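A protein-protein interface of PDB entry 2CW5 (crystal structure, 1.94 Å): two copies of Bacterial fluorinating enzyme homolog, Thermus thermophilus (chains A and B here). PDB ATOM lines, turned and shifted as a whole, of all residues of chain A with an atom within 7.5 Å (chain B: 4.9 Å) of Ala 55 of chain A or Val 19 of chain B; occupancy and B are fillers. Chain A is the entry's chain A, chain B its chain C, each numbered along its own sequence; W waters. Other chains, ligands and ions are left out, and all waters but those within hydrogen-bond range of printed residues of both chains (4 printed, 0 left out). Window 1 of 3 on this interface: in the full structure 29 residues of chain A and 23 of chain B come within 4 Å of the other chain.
OH of Tyr 58 of chain A lies close to NE of Arg 135 of chain B, at 3.4 Å.
No position is printed for both chains.
Of the 13 pairs that touch across the chains among the printed residues, none has its exchanged pair printed and touching as well.
O of Leu 59 of chain A sits at hydrogen-bond distance from NE1 of Trp 86 of chain A, at 3.0 Å.
Of the 20 printed residues of chain A, 9 touch a printed residue of chain B.
Printed residues of chain A that touch a printed residue of chain B: Tyr 5, Val 34, Asp 35, Leu 36, Ala 51, Glu 54, Ala 55, Tyr 58 and Leu 59.
Of the printed residues of chain B, Val 34 of chain A touches Ala 18 and Lys 21.
Ala 55 of chain A touches one residue of chain B.
Pro 60 of chain A touches none of the printed residues of chain B.
Val 17 of chain B touches none of the printed residues of chain A.
Ala 18 of chain B touches just these residues of chain A: Val 34 (3.9 Å), Asp 35 (3.4 Å) and Leu 36 (3.7 Å).
Val 19 of chain B touches just one residue of chain A: Ala 55 (3.7 Å).
Printed residues of chain A within 4 Å of Ala 22 of chain B: Tyr 5, Tyr 58 and Leu 59.
Of the printed residues of chain A, Arg 135 of chain B touches Tyr 58 (3.2 Å).
The nearest printed residue of chain A that does not touch Tyr 16 of chain B is Leu 36 of chain A (5.0 Å).
Water W1 lies within hydrogen-bond range of O of Leu 36 of chain A (2.5 Å), N of Ala 18 of chain B (3.0 Å) and N of Val 17 of chain B (3.3 Å).
Water W2 bridges the backbone carbonyl oxygen of Asp 35 of chain A (2.8 Å) and the side-chain amino group of Lys 21 of chain B (3.1 Å).
Water W4 bridges the guanidinium group of Arg 135 of chain B (2.9 Å) and the backbone carbonyl oxygen of Glu 54 of chain A (3.0 Å).
Water W3 bridges OE2 of Glu 54 of chain A (3.4 Å) and NH1 of Arg 135 of chain B (3.4 Å).
OH of Tyr 5 of chain A touches CA of Ala 22 of chain B, 3.6 Å away.
Ala 18 of chain B touches Val 34 of chain A.
CB of Ala 18 of chain B touches O of Asp 35 of chain A, at 3.4 Å.
Pro 15 of chain B touches Leu 36 of chain A.
Leu 36 of chain A touches Ala 18 of chain B.
O of Ala 51 of chain A touches CG of Pro 15 of chain B, 3.6 Å away.
Glu 54 of chain A touches Tyr 16 of chain B.
CB of Ala 55 of chain A touches CG2 of Val 19 of chain B (3.7 Å).
Tyr 58 of chain A touches Ala 22 of chain B (O to CB, 3.3 Å).
Ala 22 of chain B touches Leu 59 of chain A (CB to CD2, 3.9 Å).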
ATOM      1  N   TYR A   5      11.863   9.312 -33.254  1.00  0.00           N
ATOM      2  CA  TYR A   5      12.987   8.621 -32.637  1.00  0.00           C
ATOM      3  C   TYR A   5      13.354   7.528 -33.628  1.00  0.00           C
ATOM      4  O   TYR A   5      12.532   6.672 -33.961  1.00  0.00           O
ATOM      5  CB  TYR A   5      12.576   8.073 -31.277  1.00  0.00           C
ATOM      6  CG  TYR A   5      12.574   9.163 -30.225  1.00  0.00           C
ATOM      7  CD1 TYR A   5      13.680   9.367 -29.408  1.00  0.00           C
ATOM      8  CD2 TYR A   5      11.484  10.024 -30.084  1.00  0.00           C
ATOM      9  CE1 TYR A   5      13.704  10.398 -28.475  1.00  0.00           C
ATOM     10  CE2 TYR A   5      11.501  11.061 -29.151  1.00  0.00           C
ATOM     11  CZ  TYR A   5      12.614  11.238 -28.350  1.00  0.00           C
ATOM     12  OH  TYR A   5      12.634  12.237 -27.405  1.00  0.00           O
ATOM     13  N   LEU A   7      15.814   4.375 -35.029  1.00  0.00           N
ATOM     14  CA  LEU A   7      16.686   3.246 -34.717  1.00  0.00           C
ATOM     15  C   LEU A   7      16.960   2.377 -35.951  1.00  0.00           C
ATOM     16  O   LEU A   7      16.095   2.212 -36.815  1.00  0.00           O
ATOM     17  CB  LEU A   7      16.050   2.391 -33.615  1.00  0.00           C
ATOM     18  CG  LEU A   7      16.820   1.144 -33.164  1.00  0.00           C
ATOM     19  CD1 LEU A   7      16.684   0.972 -31.675  1.00  0.00           C
ATOM     20  CD2 LEU A   7      16.300  -0.077 -33.884  1.00  0.00           C
ATOM     21  N   VAL A  34      15.520  12.368 -33.185  1.00  0.00           N
ATOM     22  CA  VAL A  34      16.497  11.877 -32.231  1.00  0.00           C
ATOM     23  C   VAL A  34      16.882  10.446 -32.571  1.00  0.00           C
ATOM     24  O   VAL A  34      16.012   9.597 -32.755  1.00  0.00           O
ATOM     25  CB  VAL A  34      15.924  11.908 -30.795  1.00  0.00           C
ATOM     26  CG1 VAL A  34      16.929  11.302 -29.822  1.00  0.00           C
ATOM     27  CG2 VAL A  34      15.589  13.338 -30.402  1.00  0.00           C
ATOM     28  N   ASP A  35      18.180  10.181 -32.662  1.00  0.00           N
ATOM     29  CA  ASP A  35      18.635   8.835 -32.964  1.00  0.00           C
ATOM     30  C   ASP A  35      18.623   7.985 -31.704  1.00  0.00           C
ATOM     31  O   ASP A  35      19.190   8.374 -30.687  1.00  0.00           O
ATOM     32  CB  ASP A  35      20.065   8.823 -33.513  1.00  0.00           C
ATOM     33  CG  ASP A  35      20.179   9.435 -34.888  1.00  0.00           C
ATOM     34  OD1 ASP A  35      19.316   9.163 -35.755  1.00  0.00           O
ATOM     35  OD2 ASP A  35      21.155  10.174 -35.104  1.00  0.00           O
ATOM     36  N   LEU A  36      17.967   6.832 -31.768  1.00  0.00           N
ATOM     37  CA  LEU A  36      17.945   5.913 -30.631  1.00  0.00           C
ATOM     38  C   LEU A  36      19.310   5.220 -30.655  1.00  0.00           C
ATOM     39  O   LEU A  36      20.036   5.209 -29.659  1.00  0.00           O
ATOM     40  CB  LEU A  36      16.799   4.903 -30.793  1.00  0.00           C
ATOM     41  CG  LEU A  36      15.418   5.516 -30.519  1.00  0.00           C
ATOM     42  CD1 LEU A  36      14.292   4.669 -31.116  1.00  0.00           C
ATOM     43  CD2 LEU A  36      15.246   5.650 -29.009  1.00  0.00           C
ATOM     44  N   ALA A  49      14.835  -5.140 -30.601  1.00  0.00           N
ATOM     45  CA  ALA A  49      13.550  -5.191 -29.918  1.00  0.00           C
ATOM     46  C   ALA A  49      13.721  -4.731 -28.467  1.00  0.00           C
ATOM     47  O   ALA A  49      12.908  -3.969 -27.940  1.00  0.00           O
ATOM     48  CB  ALA A  49      12.993  -6.620 -29.967  1.00  0.00           C
ATOM     49  N   TYR A  50      14.795  -5.180 -27.829  1.00  0.00           N
ATOM     50  CA  TYR A  50      15.049  -4.796 -26.442  1.00  0.00           C
ATOM     51  C   TYR A  50      15.364  -3.297 -26.318  1.00  0.00           C
ATOM     52  O   TYR A  50      14.895  -2.632 -25.396  1.00  0.00           O
ATOM     53  CB  TYR A  50      16.204  -5.621 -25.867  1.00  0.00           C
ATOM     54  CG  TYR A  50      16.513  -5.267 -24.432  1.00  0.00           C
ATOM     55  CD1 TYR A  50      15.536  -5.378 -23.441  1.00  0.00           C
ATOM     56  CD2 TYR A  50      17.763  -4.774 -24.075  1.00  0.00           C
ATOM     57  CE1 TYR A  50      15.798  -5.000 -22.133  1.00  0.00           C
ATOM     58  CE2 TYR A  50      18.037  -4.393 -22.769  1.00  0.00           C
ATOM     59  CZ  TYR A  50      17.055  -4.507 -21.807  1.00  0.00           C
ATOM     60  OH  TYR A  50      17.330  -4.125 -20.520  1.00  0.00           O
ATOM     61  N   ALA A  51      16.157  -2.766 -27.246  1.00  0.00           N
ATOM     62  CA  ALA A  51      16.501  -1.345 -27.208  1.00  0.00           C
ATOM     63  C   ALA A  51      15.218  -0.521 -27.206  1.00  0.00           C
ATOM     64  O   ALA A  51      15.093   0.461 -26.472  1.00  0.00           O
ATOM     65  CB  ALA A  51      17.358  -0.977 -28.411  1.00  0.00           C
ATOM     66  N   LEU A  52      14.256  -0.926 -28.024  1.00  0.00           N
ATOM     67  CA  LEU A  52      12.984  -0.218 -28.091  1.00  0.00           C
ATOM     68  C   LEU A  52      12.253  -0.341 -26.756  1.00  0.00           C
ATOM     69  O   LEU A  52      11.686   0.630 -26.261  1.00  0.00           O
ATOM     70  CB  LEU A  52      12.125  -0.782 -29.228  1.00  0.00           C
ATOM     71  CG  LEU A  52      12.697  -0.538 -30.631  1.00  0.00           C
ATOM     72  CD1 LEU A  52      11.766  -1.141 -31.678  1.00  0.00           C
ATOM     73  CD2 LEU A  52      12.867   0.963 -30.864  1.00  0.00           C
ATOM     74  N   PHE A  53      12.278  -1.539 -26.175  1.00  0.00           N
ATOM     75  CA  PHE A  53      11.639  -1.787 -24.883  1.00  0.00           C
ATOM     76  C   PHE A  53      12.252  -0.877 -23.812  1.00  0.00           C
ATOM     77  O   PHE A  53      11.540  -0.293 -22.994  1.00  0.00           O
ATOM     78  CB  PHE A  53      11.839  -3.255 -24.483  1.00  0.00           C
ATOM     79  CG  PHE A  53      11.215  -3.623 -23.162  1.00  0.00           C
ATOM     80  CD1 PHE A  53       9.839  -3.810 -23.049  1.00  0.00           C
ATOM     81  CD2 PHE A  53      12.009  -3.805 -22.033  1.00  0.00           C
ATOM     82  CE1 PHE A  53       9.264  -4.174 -21.834  1.00  0.00           C
ATOM     83  CE2 PHE A  53      11.448  -4.169 -20.813  1.00  0.00           C
ATOM     84  CZ  PHE A  53      10.065  -4.356 -20.715  1.00  0.00           C
ATOM     85  N   GLU A  54      13.580  -0.770 -23.822  1.00  0.00           N
ATOM     86  CA  GLU A  54      14.304   0.063 -22.854  1.00  0.00           C
ATOM     87  C   GLU A  54      13.910   1.532 -22.896  1.00  0.00           C
ATOM     88  O   GLU A  54      13.748   2.180 -21.863  1.00  0.00           O
ATOM     89  CB  GLU A  54      15.811   0.018 -23.120  1.00  0.00           C
ATOM     90  CG  GLU A  54      16.531  -1.250 -22.751  1.00  0.00           C
ATOM     91  CD  GLU A  54      18.025  -1.117 -22.997  1.00  0.00           C
ATOM     92  OE1 GLU A  54      18.459  -1.221 -24.170  1.00  0.00           O
ATOM     93  OE2 GLU A  54      18.755  -0.884 -22.017  1.00  0.00           O
ATOM     94  N   ALA A  55      13.783   2.059 -24.106  1.00  0.00           N
ATOM     95  CA  ALA A  55      13.489   3.474 -24.299  1.00  0.00           C
ATOM     96  C   ALA A  55      12.039   3.915 -24.257  1.00  0.00           C
ATOM     97  O   ALA A  55      11.728   4.995 -23.742  1.00  0.00           O
ATOM     98  CB  ALA A  55      14.120   3.928 -25.609  1.00  0.00           C
ATOM     99  N   LEU A  56      11.151   3.083 -24.790  1.00  0.00           N
ATOM    100  CA  LEU A  56       9.738   3.429 -24.887  1.00  0.00           C
ATOM    101  C   LEU A  56       9.063   4.149 -23.725  1.00  0.00           C
ATOM    102  O   LEU A  56       8.425   5.185 -23.932  1.00  0.00           O
ATOM    103  CB  LEU A  56       8.910   2.188 -25.251  1.00  0.00           C
ATOM    104  CG  LEU A  56       7.494   2.517 -25.746  1.00  0.00           C
ATOM    105  CD1 LEU A  56       7.589   3.376 -26.996  1.00  0.00           C
ATOM    106  CD2 LEU A  56       6.727   1.235 -26.051  1.00  0.00           C
ATOM    107  N   PRO A  57       9.181   3.617 -22.492  1.00  0.00           N
ATOM    108  CA  PRO A  57       8.544   4.254 -21.331  1.00  0.00           C
ATOM    109  C   PRO A  57       8.909   5.721 -21.101  1.00  0.00           C
ATOM    110  O   PRO A  57       8.162   6.455 -20.444  1.00  0.00           O
ATOM    111  CB  PRO A  57       8.996   3.386 -20.148  1.00  0.00           C
ATOM    112  CG  PRO A  57       9.285   2.046 -20.767  1.00  0.00           C
ATOM    113  CD  PRO A  57       9.950   2.428 -22.084  1.00  0.00           C
ATOM    114  N   TYR A  58      10.049   6.144 -21.639  1.00  0.00           N
ATOM    115  CA  TYR A  58      10.519   7.510 -21.445  1.00  0.00           C
ATOM    116  C   TYR A  58      10.321   8.446 -22.625  1.00  0.00           C
ATOM    117  O   TYR A  58      10.625   9.638 -22.531  1.00  0.00           O
ATOM    118  CB  TYR A  58      11.996   7.465 -21.055  1.00  0.00           C
ATOM    119  CG  TYR A  58      12.209   6.620 -19.825  1.00  0.00           C
ATOM    120  CD1 TYR A  58      11.929   7.126 -18.555  1.00  0.00           C
ATOM    121  CD2 TYR A  58      12.613   5.288 -19.931  1.00  0.00           C
ATOM    122  CE1 TYR A  58      12.044   6.325 -17.419  1.00  0.00           C
ATOM    123  CE2 TYR A  58      12.729   4.478 -18.805  1.00  0.00           C
ATOM    124  CZ  TYR A  58      12.443   5.004 -17.554  1.00  0.00           C
ATOM    125  OH  TYR A  58      12.550   4.212 -16.435  1.00  0.00           O
ATOM    126  N   LEU A  59       9.808   7.923 -23.733  1.00  0.00           N
ATOM    127  CA  LEU A  59       9.598   8.762 -24.905  1.00  0.00           C
ATOM    128  C   LEU A  59       8.308   9.551 -24.784  1.00  0.00           C
ATOM    129  O   LEU A  59       7.340   9.081 -24.187  1.00  0.00           O
ATOM    130  CB  LEU A  59       9.545   7.913 -26.174  1.00  0.00           C
ATOM    131  CG  LEU A  59      10.730   6.985 -26.435  1.00  0.00           C
ATOM    132  CD1 LEU A  59      10.531   6.320 -27.802  1.00  0.00           C
ATOM    133  CD2 LEU A  59      12.035   7.771 -26.411  1.00  0.00           C
ATOM    134  N   PRO A  60       8.275  10.765 -25.358  1.00  0.00           N
ATOM    135  CA  PRO A  60       7.073  11.606 -25.305  1.00  0.00           C
ATOM    136  C   PRO A  60       5.897  10.813 -25.848  1.00  0.00           C
ATOM    137  O   PRO A  60       6.038  10.120 -26.854  1.00  0.00           O
ATOM    138  CB  PRO A  60       7.417  12.767 -26.235  1.00  0.00           C
ATOM    139  CG  PRO A  60       8.904  12.855 -26.143  1.00  0.00           C
ATOM    140  CD  PRO A  60       9.330  11.410 -26.160  1.00  0.00           C
ATOM    141  N   TRP A  86       2.029   5.249 -28.513  1.00  0.00           N
ATOM    142  CA  TRP A  86       3.134   5.760 -29.302  1.00  0.00           C
ATOM    143  C   TRP A  86       2.850   5.256 -30.713  1.00  0.00           C
ATOM    144  O   TRP A  86       1.949   4.438 -30.916  1.00  0.00           O
ATOM    145  CB  TRP A  86       4.468   5.209 -28.800  1.00  0.00           C
ATOM    146  CG  TRP A  86       4.872   5.782 -27.474  1.00  0.00           C
ATOM    147  CD1 TRP A  86       5.519   6.967 -27.252  1.00  0.00           C
ATOM    148  CD2 TRP A  86       4.653   5.197 -26.185  1.00  0.00           C
ATOM    149  NE1 TRP A  86       5.722   7.152 -25.900  1.00  0.00           N
ATOM    150  CE2 TRP A  86       5.201   6.080 -25.223  1.00  0.00           C
ATOM    151  CE3 TRP A  86       4.049   4.011 -25.748  1.00  0.00           C
ATOM    152  CZ2 TRP A  86       5.162   5.814 -23.845  1.00  0.00           C
ATOM    153  CZ3 TRP A  86       4.011   3.744 -24.373  1.00  0.00           C
ATOM    154  CH2 TRP A  86       4.566   4.646 -23.443  1.00  0.00           C
ATOM    155  N   LEU A 102       4.246  -3.450 -24.038  1.00  0.00           N
ATOM    156  CA  LEU A 102       4.010  -2.280 -23.208  1.00  0.00           C
ATOM    157  C   LEU A 102       2.872  -1.442 -23.787  1.00  0.00           C
ATOM    158  O   LEU A 102       2.090  -0.831 -23.045  1.00  0.00           O
ATOM    159  CB  LEU A 102       5.276  -1.414 -23.136  1.00  0.00           C
ATOM    160  CG  LEU A 102       6.544  -2.015 -22.522  1.00  0.00           C
ATOM    161  CD1 LEU A 102       7.686  -1.023 -22.611  1.00  0.00           C
ATOM    162  CD2 LEU A 102       6.277  -2.380 -21.069  1.00  0.00           C
ATOM    163  N   ALA A 228      15.943  -1.749 -17.193  1.00  0.00           N
ATOM    164  CA  ALA A 228      14.678  -1.874 -17.911  1.00  0.00           C
ATOM    165  C   ALA A 228      13.694  -2.824 -17.231  1.00  0.00           C
ATOM    166  O   ALA A 228      12.711  -3.245 -17.836  1.00  0.00           O
ATOM    167  CB  ALA A 228      14.935  -2.331 -19.348  1.00  0.00           C
ATOM    168  N   PRO B  15      20.374   2.808 -26.674  1.00  0.00           N
ATOM    169  CA  PRO B  15      19.533   4.003 -26.768  1.00  0.00           C
ATOM    170  C   PRO B  15      19.667   4.911 -25.538  1.00  0.00           C
ATOM    171  O   PRO B  15      18.814   5.758 -25.300  1.00  0.00           O
ATOM    172  CB  PRO B  15      18.134   3.414 -26.889  1.00  0.00           C
ATOM    173  CG  PRO B  15      18.216   2.252 -25.938  1.00  0.00           C
ATOM    174  CD  PRO B  15      19.577   1.638 -26.252  1.00  0.00           C
ATOM    175  N   TYR B  16      20.738   4.745 -24.769  1.00  0.00           N
ATOM    176  CA  TYR B  16      20.919   5.554 -23.560  1.00  0.00           C
ATOM    177  C   TYR B  16      20.958   7.059 -23.813  1.00  0.00           C
ATOM    178  O   TYR B  16      20.316   7.832 -23.098  1.00  0.00           O
ATOM    179  CB  TYR B  16      22.180   5.121 -22.810  1.00  0.00           C
ATOM    180  CG  TYR B  16      22.226   3.640 -22.511  1.00  0.00           C
ATOM    181  CD1 TYR B  16      21.074   2.948 -22.134  1.00  0.00           C
ATOM    182  CD2 TYR B  16      23.423   2.930 -22.599  1.00  0.00           C
ATOM    183  CE1 TYR B  16      21.111   1.580 -21.853  1.00  0.00           C
ATOM    184  CE2 TYR B  16      23.472   1.563 -22.319  1.00  0.00           C
ATOM    185  CZ  TYR B  16      22.314   0.897 -21.951  1.00  0.00           C
ATOM    186  OH  TYR B  16      22.360  -0.454 -21.697  1.00  0.00           O
ATOM    187  N   VAL B  17      21.695   7.489 -24.831  1.00  0.00           N
ATOM    188  CA  VAL B  17      21.761   8.921 -25.122  1.00  0.00           C
ATOM    189  C   VAL B  17      20.364   9.461 -25.425  1.00  0.00           C
ATOM    190  O   VAL B  17      19.971  10.514 -24.920  1.00  0.00           O
ATOM    191  CB  VAL B  17      22.696   9.219 -26.331  1.00  0.00           C
ATOM    192  CG1 VAL B  17      22.570  10.686 -26.746  1.00  0.00           C
ATOM    193  CG2 VAL B  17      24.152   8.915 -25.954  1.00  0.00           C
ATOM    194  N   ALA B  18      19.613   8.725 -26.241  1.00  0.00           N
ATOM    195  CA  ALA B  18      18.267   9.129 -26.625  1.00  0.00           C
ATOM    196  C   ALA B  18      17.310   9.192 -25.436  1.00  0.00           C
ATOM    197  O   ALA B  18      16.451  10.068 -25.378  1.00  0.00           O
ATOM    198  CB  ALA B  18      17.722   8.180 -27.679  1.00  0.00           C
ATOM    199  N   VAL B  19      17.442   8.253 -24.500  1.00  0.00           N
ATOM    200  CA  VAL B  19      16.577   8.239 -23.326  1.00  0.00           C
ATOM    201  C   VAL B  19      16.808   9.491 -22.478  1.00  0.00           C
ATOM    202  O   VAL B  19      15.856  10.094 -21.976  1.00  0.00           O
ATOM    203  CB  VAL B  19      16.813   6.975 -22.469  1.00  0.00           C
ATOM    204  CG1 VAL B  19      16.008   7.059 -21.170  1.00  0.00           C
ATOM    205  CG2 VAL B  19      16.392   5.739 -23.253  1.00  0.00           C
ATOM    206  N   VAL B  20      18.068   9.887 -22.326  1.00  0.00           N
ATOM    207  CA  VAL B  20      18.381  11.087 -21.565  1.00  0.00           C
ATOM    208  C   VAL B  20      17.770  12.301 -22.269  1.00  0.00           C
ATOM    209  O   VAL B  20      17.198  13.187 -21.630  1.00  0.00           O
ATOM    210  CB  VAL B  20      19.904  11.275 -21.422  1.00  0.00           C
ATOM    211  CG1 VAL B  20      20.209  12.657 -20.869  1.00  0.00           C
ATOM    212  CG2 VAL B  20      20.468  10.204 -20.484  1.00  0.00           C
ATOM    213  N   LYS B  21      17.885  12.339 -23.591  1.00  0.00           N
ATOM    214  CA  LYS B  21      17.310  13.439 -24.357  1.00  0.00           C
ATOM    215  C   LYS B  21      15.783  13.439 -24.213  1.00  0.00           C
ATOM    216  O   LYS B  21      15.146  14.498 -24.190  1.00  0.00           O
ATOM    217  CB  LYS B  21      17.697  13.308 -25.832  1.00  0.00           C
ATOM    218  CG  LYS B  21      19.164  13.587 -26.113  1.00  0.00           C
ATOM    219  CD  LYS B  21      19.457  13.454 -27.602  1.00  0.00           C
ATOM    220  CE  LYS B  21      20.878  13.855 -27.927  1.00  0.00           C
ATOM    221  NZ  LYS B  21      21.165  13.662 -29.376  1.00  0.00           N
ATOM    222  N   ALA B  22      15.198  12.247 -24.117  1.00  0.00           N
ATOM    223  CA  ALA B  22      13.751  12.118 -23.966  1.00  0.00           C
ATOM    224  C   ALA B  22      13.317  12.667 -22.610  1.00  0.00           C
ATOM    225  O   ALA B  22      12.327  13.389 -22.517  1.00  0.00           O
ATOM    226  CB  ALA B  22      13.332  10.653 -24.094  1.00  0.00           C
ATOM    227  N   VAL B  23      14.056  12.321 -21.559  1.00  0.00           N
ATOM    228  CA  VAL B  23      13.723  12.816 -20.227  1.00  0.00           C
ATOM    229  C   VAL B  23      13.886  14.334 -20.198  1.00  0.00           C
ATOM    230  O   VAL B  23      13.063  15.037 -19.617  1.00  0.00           O
ATOM    231  CB  VAL B  23      14.617  12.177 -19.136  1.00  0.00           C
ATOM    232  CG1 VAL B  23      14.356  12.840 -17.790  1.00  0.00           C
ATOM    233  CG2 VAL B  23      14.322  10.687 -19.035  1.00  0.00           C
ATOM    234  N   PHE B 132      20.905   3.376 -13.821  1.00  0.00           N
ATOM    235  CA  PHE B 132      21.018   4.297 -14.951  1.00  0.00           C
ATOM    236  C   PHE B 132      20.940   5.732 -14.425  1.00  0.00           C
ATOM    237  O   PHE B 132      19.938   6.420 -14.622  1.00  0.00           O
ATOM    238  CB  PHE B 132      19.868   4.029 -15.938  1.00  0.00           C
ATOM    239  CG  PHE B 132      20.038   4.685 -17.291  1.00  0.00           C
ATOM    240  CD1 PHE B 132      21.033   5.636 -17.516  1.00  0.00           C
ATOM    241  CD2 PHE B 132      19.181   4.355 -18.338  1.00  0.00           C
ATOM    242  CE1 PHE B 132      21.172   6.250 -18.764  1.00  0.00           C
ATOM    243  CE2 PHE B 132      19.305   4.960 -19.586  1.00  0.00           C
ATOM    244  CZ  PHE B 132      20.308   5.913 -19.800  1.00  0.00           C
ATOM    245  N   ARG B 135      19.805   8.763 -16.641  1.00  0.00           N
ATOM    246  CA  ARG B 135      18.365   8.867 -16.825  1.00  0.00           C
ATOM    247  C   ARG B 135      17.612   9.323 -15.578  1.00  0.00           C
ATOM    248  O   ARG B 135      16.797  10.246 -15.632  1.00  0.00           O
ATOM    249  CB  ARG B 135      17.807   7.502 -17.244  1.00  0.00           C
ATOM    250  CG  ARG B 135      16.301   7.472 -17.475  1.00  0.00           C
ATOM    251  CD  ARG B 135      15.822   6.042 -17.699  1.00  0.00           C
ATOM    252  NE  ARG B 135      15.780   5.275 -16.453  1.00  0.00           N
ATOM    253  CZ  ARG B 135      15.767   3.946 -16.388  1.00  0.00           C
ATOM    254  NH1 ARG B 135      15.802   3.219 -17.497  1.00  0.00           N
ATOM    255  NH2 ARG B 135      15.710   3.344 -15.210  1.00  0.00           N
HETATM  256  O   HOH W   1      21.099   6.736 -28.010  1.00  0.00           O
HETATM  257  O   HOH W   2      20.487  10.644 -29.735  1.00  0.00           O
HETATM  258  O   HOH W   3      17.233   1.033 -19.710  1.00  0.00           O
HETATM  259  O   HOH W   4      16.058   3.436 -20.391  1.00  0.00           O
